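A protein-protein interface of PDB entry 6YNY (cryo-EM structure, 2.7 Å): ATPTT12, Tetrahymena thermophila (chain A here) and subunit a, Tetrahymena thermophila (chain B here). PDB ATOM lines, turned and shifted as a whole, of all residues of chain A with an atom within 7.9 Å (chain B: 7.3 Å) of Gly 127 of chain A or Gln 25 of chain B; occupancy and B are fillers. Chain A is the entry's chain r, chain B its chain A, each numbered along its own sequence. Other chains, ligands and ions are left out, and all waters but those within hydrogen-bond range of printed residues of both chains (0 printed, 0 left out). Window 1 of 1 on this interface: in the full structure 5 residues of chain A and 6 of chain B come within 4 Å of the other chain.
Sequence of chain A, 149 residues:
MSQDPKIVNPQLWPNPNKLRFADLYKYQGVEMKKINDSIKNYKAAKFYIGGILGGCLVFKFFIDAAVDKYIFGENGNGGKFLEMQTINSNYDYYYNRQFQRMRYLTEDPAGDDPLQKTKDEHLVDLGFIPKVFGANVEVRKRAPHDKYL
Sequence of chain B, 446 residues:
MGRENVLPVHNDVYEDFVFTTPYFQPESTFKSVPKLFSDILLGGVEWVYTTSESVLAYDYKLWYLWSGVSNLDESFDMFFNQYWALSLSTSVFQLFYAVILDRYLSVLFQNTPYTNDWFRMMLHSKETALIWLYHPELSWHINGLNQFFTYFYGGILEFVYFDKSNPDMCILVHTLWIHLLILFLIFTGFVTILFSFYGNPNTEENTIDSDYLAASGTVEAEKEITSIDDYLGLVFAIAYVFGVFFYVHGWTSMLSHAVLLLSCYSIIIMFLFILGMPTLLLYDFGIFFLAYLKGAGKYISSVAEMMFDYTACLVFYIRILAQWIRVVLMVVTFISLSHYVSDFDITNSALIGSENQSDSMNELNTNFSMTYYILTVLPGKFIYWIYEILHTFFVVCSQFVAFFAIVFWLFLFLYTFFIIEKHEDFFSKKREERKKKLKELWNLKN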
ATOM      1  N   HIS A 122      26.938 -33.894 -14.845  1.00  0.00           N
ATOM      2  CA  HIS A 122      28.036 -33.429 -14.012  1.00  0.00           C
ATOM      3  C   HIS A 122      27.969 -31.929 -13.774  1.00  0.00           C
ATOM      4  O   HIS A 122      28.253 -31.465 -12.666  1.00  0.00           O
ATOM      5  CB  HIS A 122      29.366 -33.798 -14.672  1.00  0.00           C
ATOM      6  CG  HIS A 122      30.555 -33.632 -13.784  1.00  0.00           C
ATOM      7  ND1 HIS A 122      30.458 -33.547 -12.413  1.00  0.00           N
ATOM      8  CD2 HIS A 122      31.874 -33.540 -14.073  1.00  0.00           C
ATOM      9  CE1 HIS A 122      31.666 -33.408 -11.896  1.00  0.00           C
ATOM     10  NE2 HIS A 122      32.542 -33.400 -12.883  1.00  0.00           N
ATOM     11  N   LEU A 123      27.596 -31.162 -14.799  1.00  0.00           N
ATOM     12  CA  LEU A 123      27.457 -29.721 -14.638  1.00  0.00           C
ATOM     13  C   LEU A 123      26.418 -29.375 -13.585  1.00  0.00           C
ATOM     14  O   LEU A 123      26.565 -28.379 -12.870  1.00  0.00           O
ATOM     15  CB  LEU A 123      27.085 -29.082 -15.973  1.00  0.00           C
ATOM     16  CG  LEU A 123      28.152 -29.088 -17.061  1.00  0.00           C
ATOM     17  CD1 LEU A 123      27.573 -28.579 -18.361  1.00  0.00           C
ATOM     18  CD2 LEU A 123      29.327 -28.242 -16.646  1.00  0.00           C
ATOM     19  N   VAL A 124      25.359 -30.176 -13.484  1.00  0.00           N
ATOM     20  CA  VAL A 124      24.344 -29.944 -12.463  1.00  0.00           C
ATOM     21  C   VAL A 124      24.963 -30.026 -11.076  1.00  0.00           C
ATOM     22  O   VAL A 124      24.779 -29.136 -10.238  1.00  0.00           O
ATOM     23  CB  VAL A 124      23.193 -30.952 -12.623  1.00  0.00           C
ATOM     24  CG1 VAL A 124      22.280 -30.916 -11.417  1.00  0.00           C
ATOM     25  CG2 VAL A 124      22.422 -30.665 -13.886  1.00  0.00           C
ATOM     26  N   ASP A 125      25.709 -31.096 -10.813  1.00  0.00           N
ATOM     27  CA  ASP A 125      26.342 -31.278  -9.517  1.00  0.00           C
ATOM     28  C   ASP A 125      27.496 -30.315  -9.286  1.00  0.00           C
ATOM     29  O   ASP A 125      28.001 -30.245  -8.161  1.00  0.00           O
ATOM     30  CB  ASP A 125      26.831 -32.717  -9.386  1.00  0.00           C
ATOM     31  CG  ASP A 125      25.706 -33.725  -9.501  1.00  0.00           C
ATOM     32  OD1 ASP A 125      24.549 -33.303  -9.705  1.00  0.00           O
ATOM     33  OD2 ASP A 125      25.974 -34.938  -9.386  1.00  0.00           O
ATOM     34  N   LEU A 126      27.924 -29.585 -10.311  1.00  0.00           N
ATOM     35  CA  LEU A 126      28.978 -28.594 -10.163  1.00  0.00           C
ATOM     36  C   LEU A 126      28.440 -27.199  -9.895  1.00  0.00           C
ATOM     37  O   LEU A 126      29.205 -26.332  -9.463  1.00  0.00           O
ATOM     38  CB  LEU A 126      29.859 -28.566 -11.414  1.00  0.00           C
ATOM     39  CG  LEU A 126      30.769 -29.779 -11.606  1.00  0.00           C
ATOM     40  CD1 LEU A 126      31.430 -29.761 -12.962  1.00  0.00           C
ATOM     41  CD2 LEU A 126      31.813 -29.831 -10.522  1.00  0.00           C
ATOM     42  N   GLY A 127      27.154 -26.966 -10.136  1.00  0.00           N
ATOM     43  CA  GLY A 127      26.525 -25.688  -9.851  1.00  0.00           C
ATOM     44  C   GLY A 127      25.962 -24.971 -11.056  1.00  0.00           C
ATOM     45  O   GLY A 127      25.414 -23.872 -10.895  1.00  0.00           O
ATOM     46  N   PHE A 128      26.062 -25.535 -12.254  1.00  0.00           N
ATOM     47  CA  PHE A 128      25.548 -24.921 -13.469  1.00  0.00           C
ATOM     48  C   PHE A 128      24.532 -25.858 -14.100  1.00  0.00           C
ATOM     49  O   PHE A 128      24.869 -26.989 -14.461  1.00  0.00           O
ATOM     50  CB  PHE A 128      26.680 -24.627 -14.452  1.00  0.00           C
ATOM     51  CG  PHE A 128      27.532 -23.452 -14.076  1.00  0.00           C
ATOM     52  CD1 PHE A 128      26.964 -22.261 -13.677  1.00  0.00           C
ATOM     53  CD2 PHE A 128      28.907 -23.542 -14.129  1.00  0.00           C
ATOM     54  CE1 PHE A 128      27.749 -21.187 -13.340  1.00  0.00           C
ATOM     55  CE2 PHE A 128      29.696 -22.471 -13.791  1.00  0.00           C
ATOM     56  CZ  PHE A 128      29.118 -21.294 -13.396  1.00  0.00           C
ATOM     57  N   ILE A 129      23.296 -25.388 -14.229  1.00  0.00           N
ATOM     58  CA  ILE A 129      22.235 -26.138 -14.894  1.00  0.00           C
ATOM     59  C   ILE A 129      22.228 -25.728 -16.365  1.00  0.00           C
ATOM     60  O   ILE A 129      21.829 -24.593 -16.675  1.00  0.00           O
ATOM     61  CB  ILE A 129      20.874 -25.885 -14.241  1.00  0.00           C
ATOM     62  CG1 ILE A 129      20.870 -26.459 -12.826  1.00  0.00           C
ATOM     63  CG2 ILE A 129      19.770 -26.494 -15.083  1.00  0.00           C
ATOM     64  CD1 ILE A 129      19.623 -26.158 -12.043  1.00  0.00           C
ATOM     65  N   PRO A 130      22.648 -26.593 -17.285  1.00  0.00           N
ATOM     66  CA  PRO A 130      22.687 -26.200 -18.695  1.00  0.00           C
ATOM     67  C   PRO A 130      21.299 -25.949 -19.252  1.00  0.00           C
ATOM     68  O   PRO A 130      20.308 -26.535 -18.812  1.00  0.00           O
ATOM     69  CB  PRO A 130      23.344 -27.402 -19.383  1.00  0.00           C
ATOM     70  CG  PRO A 130      23.995 -28.166 -18.306  1.00  0.00           C
ATOM     71  CD  PRO A 130      23.171 -27.953 -17.093  1.00  0.00           C
ATOM     72  N   PRO B  22      24.695 -19.894 -16.387  1.00  0.00           N
ATOM     73  CA  PRO B  22      23.594 -19.835 -15.424  1.00  0.00           C
ATOM     74  C   PRO B  22      24.097 -19.457 -14.040  1.00  0.00           C
ATOM     75  O   PRO B  22      25.297 -19.403 -13.766  1.00  0.00           O
ATOM     76  CB  PRO B  22      23.014 -21.249 -15.452  1.00  0.00           C
ATOM     77  CG  PRO B  22      24.111 -22.103 -15.959  1.00  0.00           C
ATOM     78  CD  PRO B  22      24.913 -21.259 -16.888  1.00  0.00           C
ATOM     79  N   TYR B  23      23.143 -19.187 -13.158  1.00  0.00           N
ATOM     80  CA  TYR B  23      23.472 -18.785 -11.799  1.00  0.00           C
ATOM     81  C   TYR B  23      24.171 -19.922 -11.070  1.00  0.00           C
ATOM     82  O   TYR B  23      23.639 -21.032 -10.975  1.00  0.00           O
ATOM     83  CB  TYR B  23      22.202 -18.372 -11.061  1.00  0.00           C
ATOM     84  CG  TYR B  23      22.441 -17.769  -9.701  1.00  0.00           C
ATOM     85  CD1 TYR B  23      22.791 -16.434  -9.564  1.00  0.00           C
ATOM     86  CD2 TYR B  23      22.307 -18.531  -8.550  1.00  0.00           C
ATOM     87  CE1 TYR B  23      23.008 -15.877  -8.322  1.00  0.00           C
ATOM     88  CE2 TYR B  23      22.521 -17.986  -7.305  1.00  0.00           C
ATOM     89  CZ  TYR B  23      22.872 -16.656  -7.195  1.00  0.00           C
ATOM     90  OH  TYR B  23      23.087 -16.104  -5.953  1.00  0.00           O
ATOM     91  N   PHE B  24      25.366 -19.645 -10.561  1.00  0.00           N
ATOM     92  CA  PHE B  24      26.145 -20.654  -9.863  1.00  0.00           C
ATOM     93  C   PHE B  24      25.580 -20.893  -8.472  1.00  0.00           C
ATOM     94  O   PHE B  24      25.207 -19.952  -7.766  1.00  0.00           O
ATOM     95  CB  PHE B  24      27.608 -20.225  -9.773  1.00  0.00           C
ATOM     96  CG  PHE B  24      28.492 -21.230  -9.108  1.00  0.00           C
ATOM     97  CD1 PHE B  24      28.727 -22.457  -9.694  1.00  0.00           C
ATOM     98  CD2 PHE B  24      29.098 -20.946  -7.901  1.00  0.00           C
ATOM     99  CE1 PHE B  24      29.538 -23.381  -9.085  1.00  0.00           C
ATOM    100  CE2 PHE B  24      29.913 -21.872  -7.289  1.00  0.00           C
ATOM    101  CZ  PHE B  24      30.132 -23.090  -7.883  1.00  0.00           C
ATOM    102  N   GLN B  25      25.510 -22.163  -8.084  1.00  0.00           N
ATOM    103  CA  GLN B  25      25.012 -22.552  -6.769  1.00  0.00           C
ATOM    104  C   GLN B  25      26.175 -23.017  -5.905  1.00  0.00           C
ATOM    105  O   GLN B  25      26.632 -24.162  -6.045  1.00  0.00           O
ATOM    106  CB  GLN B  25      23.965 -23.660  -6.904  1.00  0.00           C
ATOM    107  CG  GLN B  25      22.782 -23.261  -7.759  1.00  0.00           C
ATOM    108  CD  GLN B  25      21.842 -24.412  -8.033  1.00  0.00           C
ATOM    109  OE1 GLN B  25      21.614 -25.264  -7.176  1.00  0.00           O
ATOM    110  NE2 GLN B  25      21.301 -24.450  -9.244  1.00  0.00           N
ATOM    111  N   PRO B  26      26.692 -22.179  -5.004  1.00  0.00           N
ATOM    112  CA  PRO B  26      27.833 -22.604  -4.180  1.00  0.00           C
ATOM    113  C   PRO B  26      27.537 -23.785  -3.277  1.00  0.00           C
ATOM    114  O   PRO B  26      28.479 -24.450  -2.828  1.00  0.00           O
ATOM    115  CB  PRO B  26      28.157 -21.346  -3.362  1.00  0.00           C
ATOM    116  CG  PRO B  26      27.580 -20.223  -4.137  1.00  0.00           C
ATOM    117  CD  PRO B  26      26.351 -20.766  -4.779  1.00  0.00           C
ATOM    118  N   GLU B  27      26.266 -24.071  -2.993  1.00  0.00           N
ATOM    119  CA  GLU B  27      25.932 -25.190  -2.120  1.00  0.00           C
ATOM    120  C   GLU B  27      26.400 -26.521  -2.689  1.00  0.00           C
ATOM    121  O   GLU B  27      26.581 -27.479  -1.931  1.00  0.00           O
ATOM    122  CB  GLU B  27      24.423 -25.222  -1.875  1.00  0.00           C
ATOM    123  CG  GLU B  27      23.960 -26.312  -0.919  1.00  0.00           C
ATOM    124  CD  GLU B  27      24.556 -26.168   0.469  1.00  0.00           C
ATOM    125  OE1 GLU B  27      25.114 -25.095   0.773  1.00  0.00           O
ATOM    126  OE2 GLU B  27      24.465 -27.134   1.256  1.00  0.00           O
ATOM    127  N   SER B  28      26.600 -26.600  -4.004  1.00  0.00           N
ATOM    128  CA  SER B  28      27.092 -27.828  -4.614  1.00  0.00           C
ATOM    129  C   SER B  28      28.492 -28.190  -4.144  1.00  0.00           C
ATOM    130  O   SER B  28      28.929 -29.327  -4.351  1.00  0.00           O
ATOM    131  CB  SER B  28      27.083 -27.683  -6.134  1.00  0.00           C
ATOM    132  OG  SER B  28      27.882 -26.588  -6.537  1.00  0.00           O
ATOM    133  N   THR B  29      29.206 -27.254  -3.518  1.00  0.00           N
ATOM    134  CA  THR B  29      30.567 -27.531  -3.078  1.00  0.00           C
ATOM    135  C   THR B  29      30.593 -28.617  -2.010  1.00  0.00           C
ATOM    136  O   THR B  29      31.368 -29.575  -2.098  1.00  0.00           O
ATOM    137  CB  THR B  29      31.210 -26.249  -2.551  1.00  0.00           C
ATOM    138  OG1 THR B  29      31.101 -25.216  -3.535  1.00  0.00           O
ATOM    139  CG2 THR B  29      32.669 -26.477  -2.228  1.00  0.00           C
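The backbone NH (N) of Gln 25 of chain B sits at hydrogen-bond distance from the backbone carbonyl oxygen (O) of Gly 127 of chain A (3.3 Å). O of Leu 126 of chain A sits at hydrogen-bond distance from OG of Ser 28 of chain B. The backbone carbonyl oxygen (O) of Gly 127 of chain A sits close to the backbone carbonyl oxygen (O) of Tyr 23 of chain B, 3.4 Å away.
The backbone carbonyl oxygen (O) of Gln 25 of chain B sits at hydrogen-bond distance from the side-chain hydroxyl (OG) of Ser 28 of chain B, at 2.8 Å. The backbone carbonyl oxygen (O) of Leu 123 of chain A is in hydrogen-bond range of the backbone NH (N) of Phe 128 of chain A (3.0 Å).
Among the printed residues, pairs that only touch across the chains: Leu 126 of chain A with Phe 24 of chain B, Phe 128 of chain A with Pro 22 of chain B, Asp 125 of chain A with Ser 28 of chain B, Ile 129 of chain A with Pro 22 of chain B, Gly 127 of chain A with Phe 24 of chain B, Ile 129 of chain A with Gln 25 of chain B, Gly 127 of chain A with Ser 28 of chain B and Phe 128 of chain A with Phe 24 of chain B.
Gly 127 of chain A touches four residues of chain B. Of chain A, only Gly 127 (3.3 Å) and Ile 129 (3.7 Å) come within 4 Å of Gln 25 of chain B. No residue of chain A comes within 4 Å of Pro 26 of chain B. Printed residues of chain B within 4 Å of Asp 125 of chain A: Ser 28. Of the printed residues of chain B, Phe 128 of chain A touches Pro 22 (3.1 Å) and Phe 24 (3.7 Å). Of the printed residues of chain B, Ile 129 of chain A touches Pro 22 and Gln 25. Pro 130 of chain A touches none of the printed residues of chain B. Glu 27 of chain B touches none of the printed residues of chain A. The nearest residue of chain B that does not touch Gly 127 of chain A is Pro 22 of chain B (5.3 Å).
Of the 8 printed residues of chain B, 5 touch a printed residue of chain A. Hydrophobic or aromatic side chains of chain A within 4 Å of the printed part of chain B: Phe 128 and Ile 129. Among the printed residues, 11 pairs touch across the chains. Among the printed residues, no Asp or Glu carboxylate lies within 4 Å of a Lys or Arg side-chain nitrogen of the other chain.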
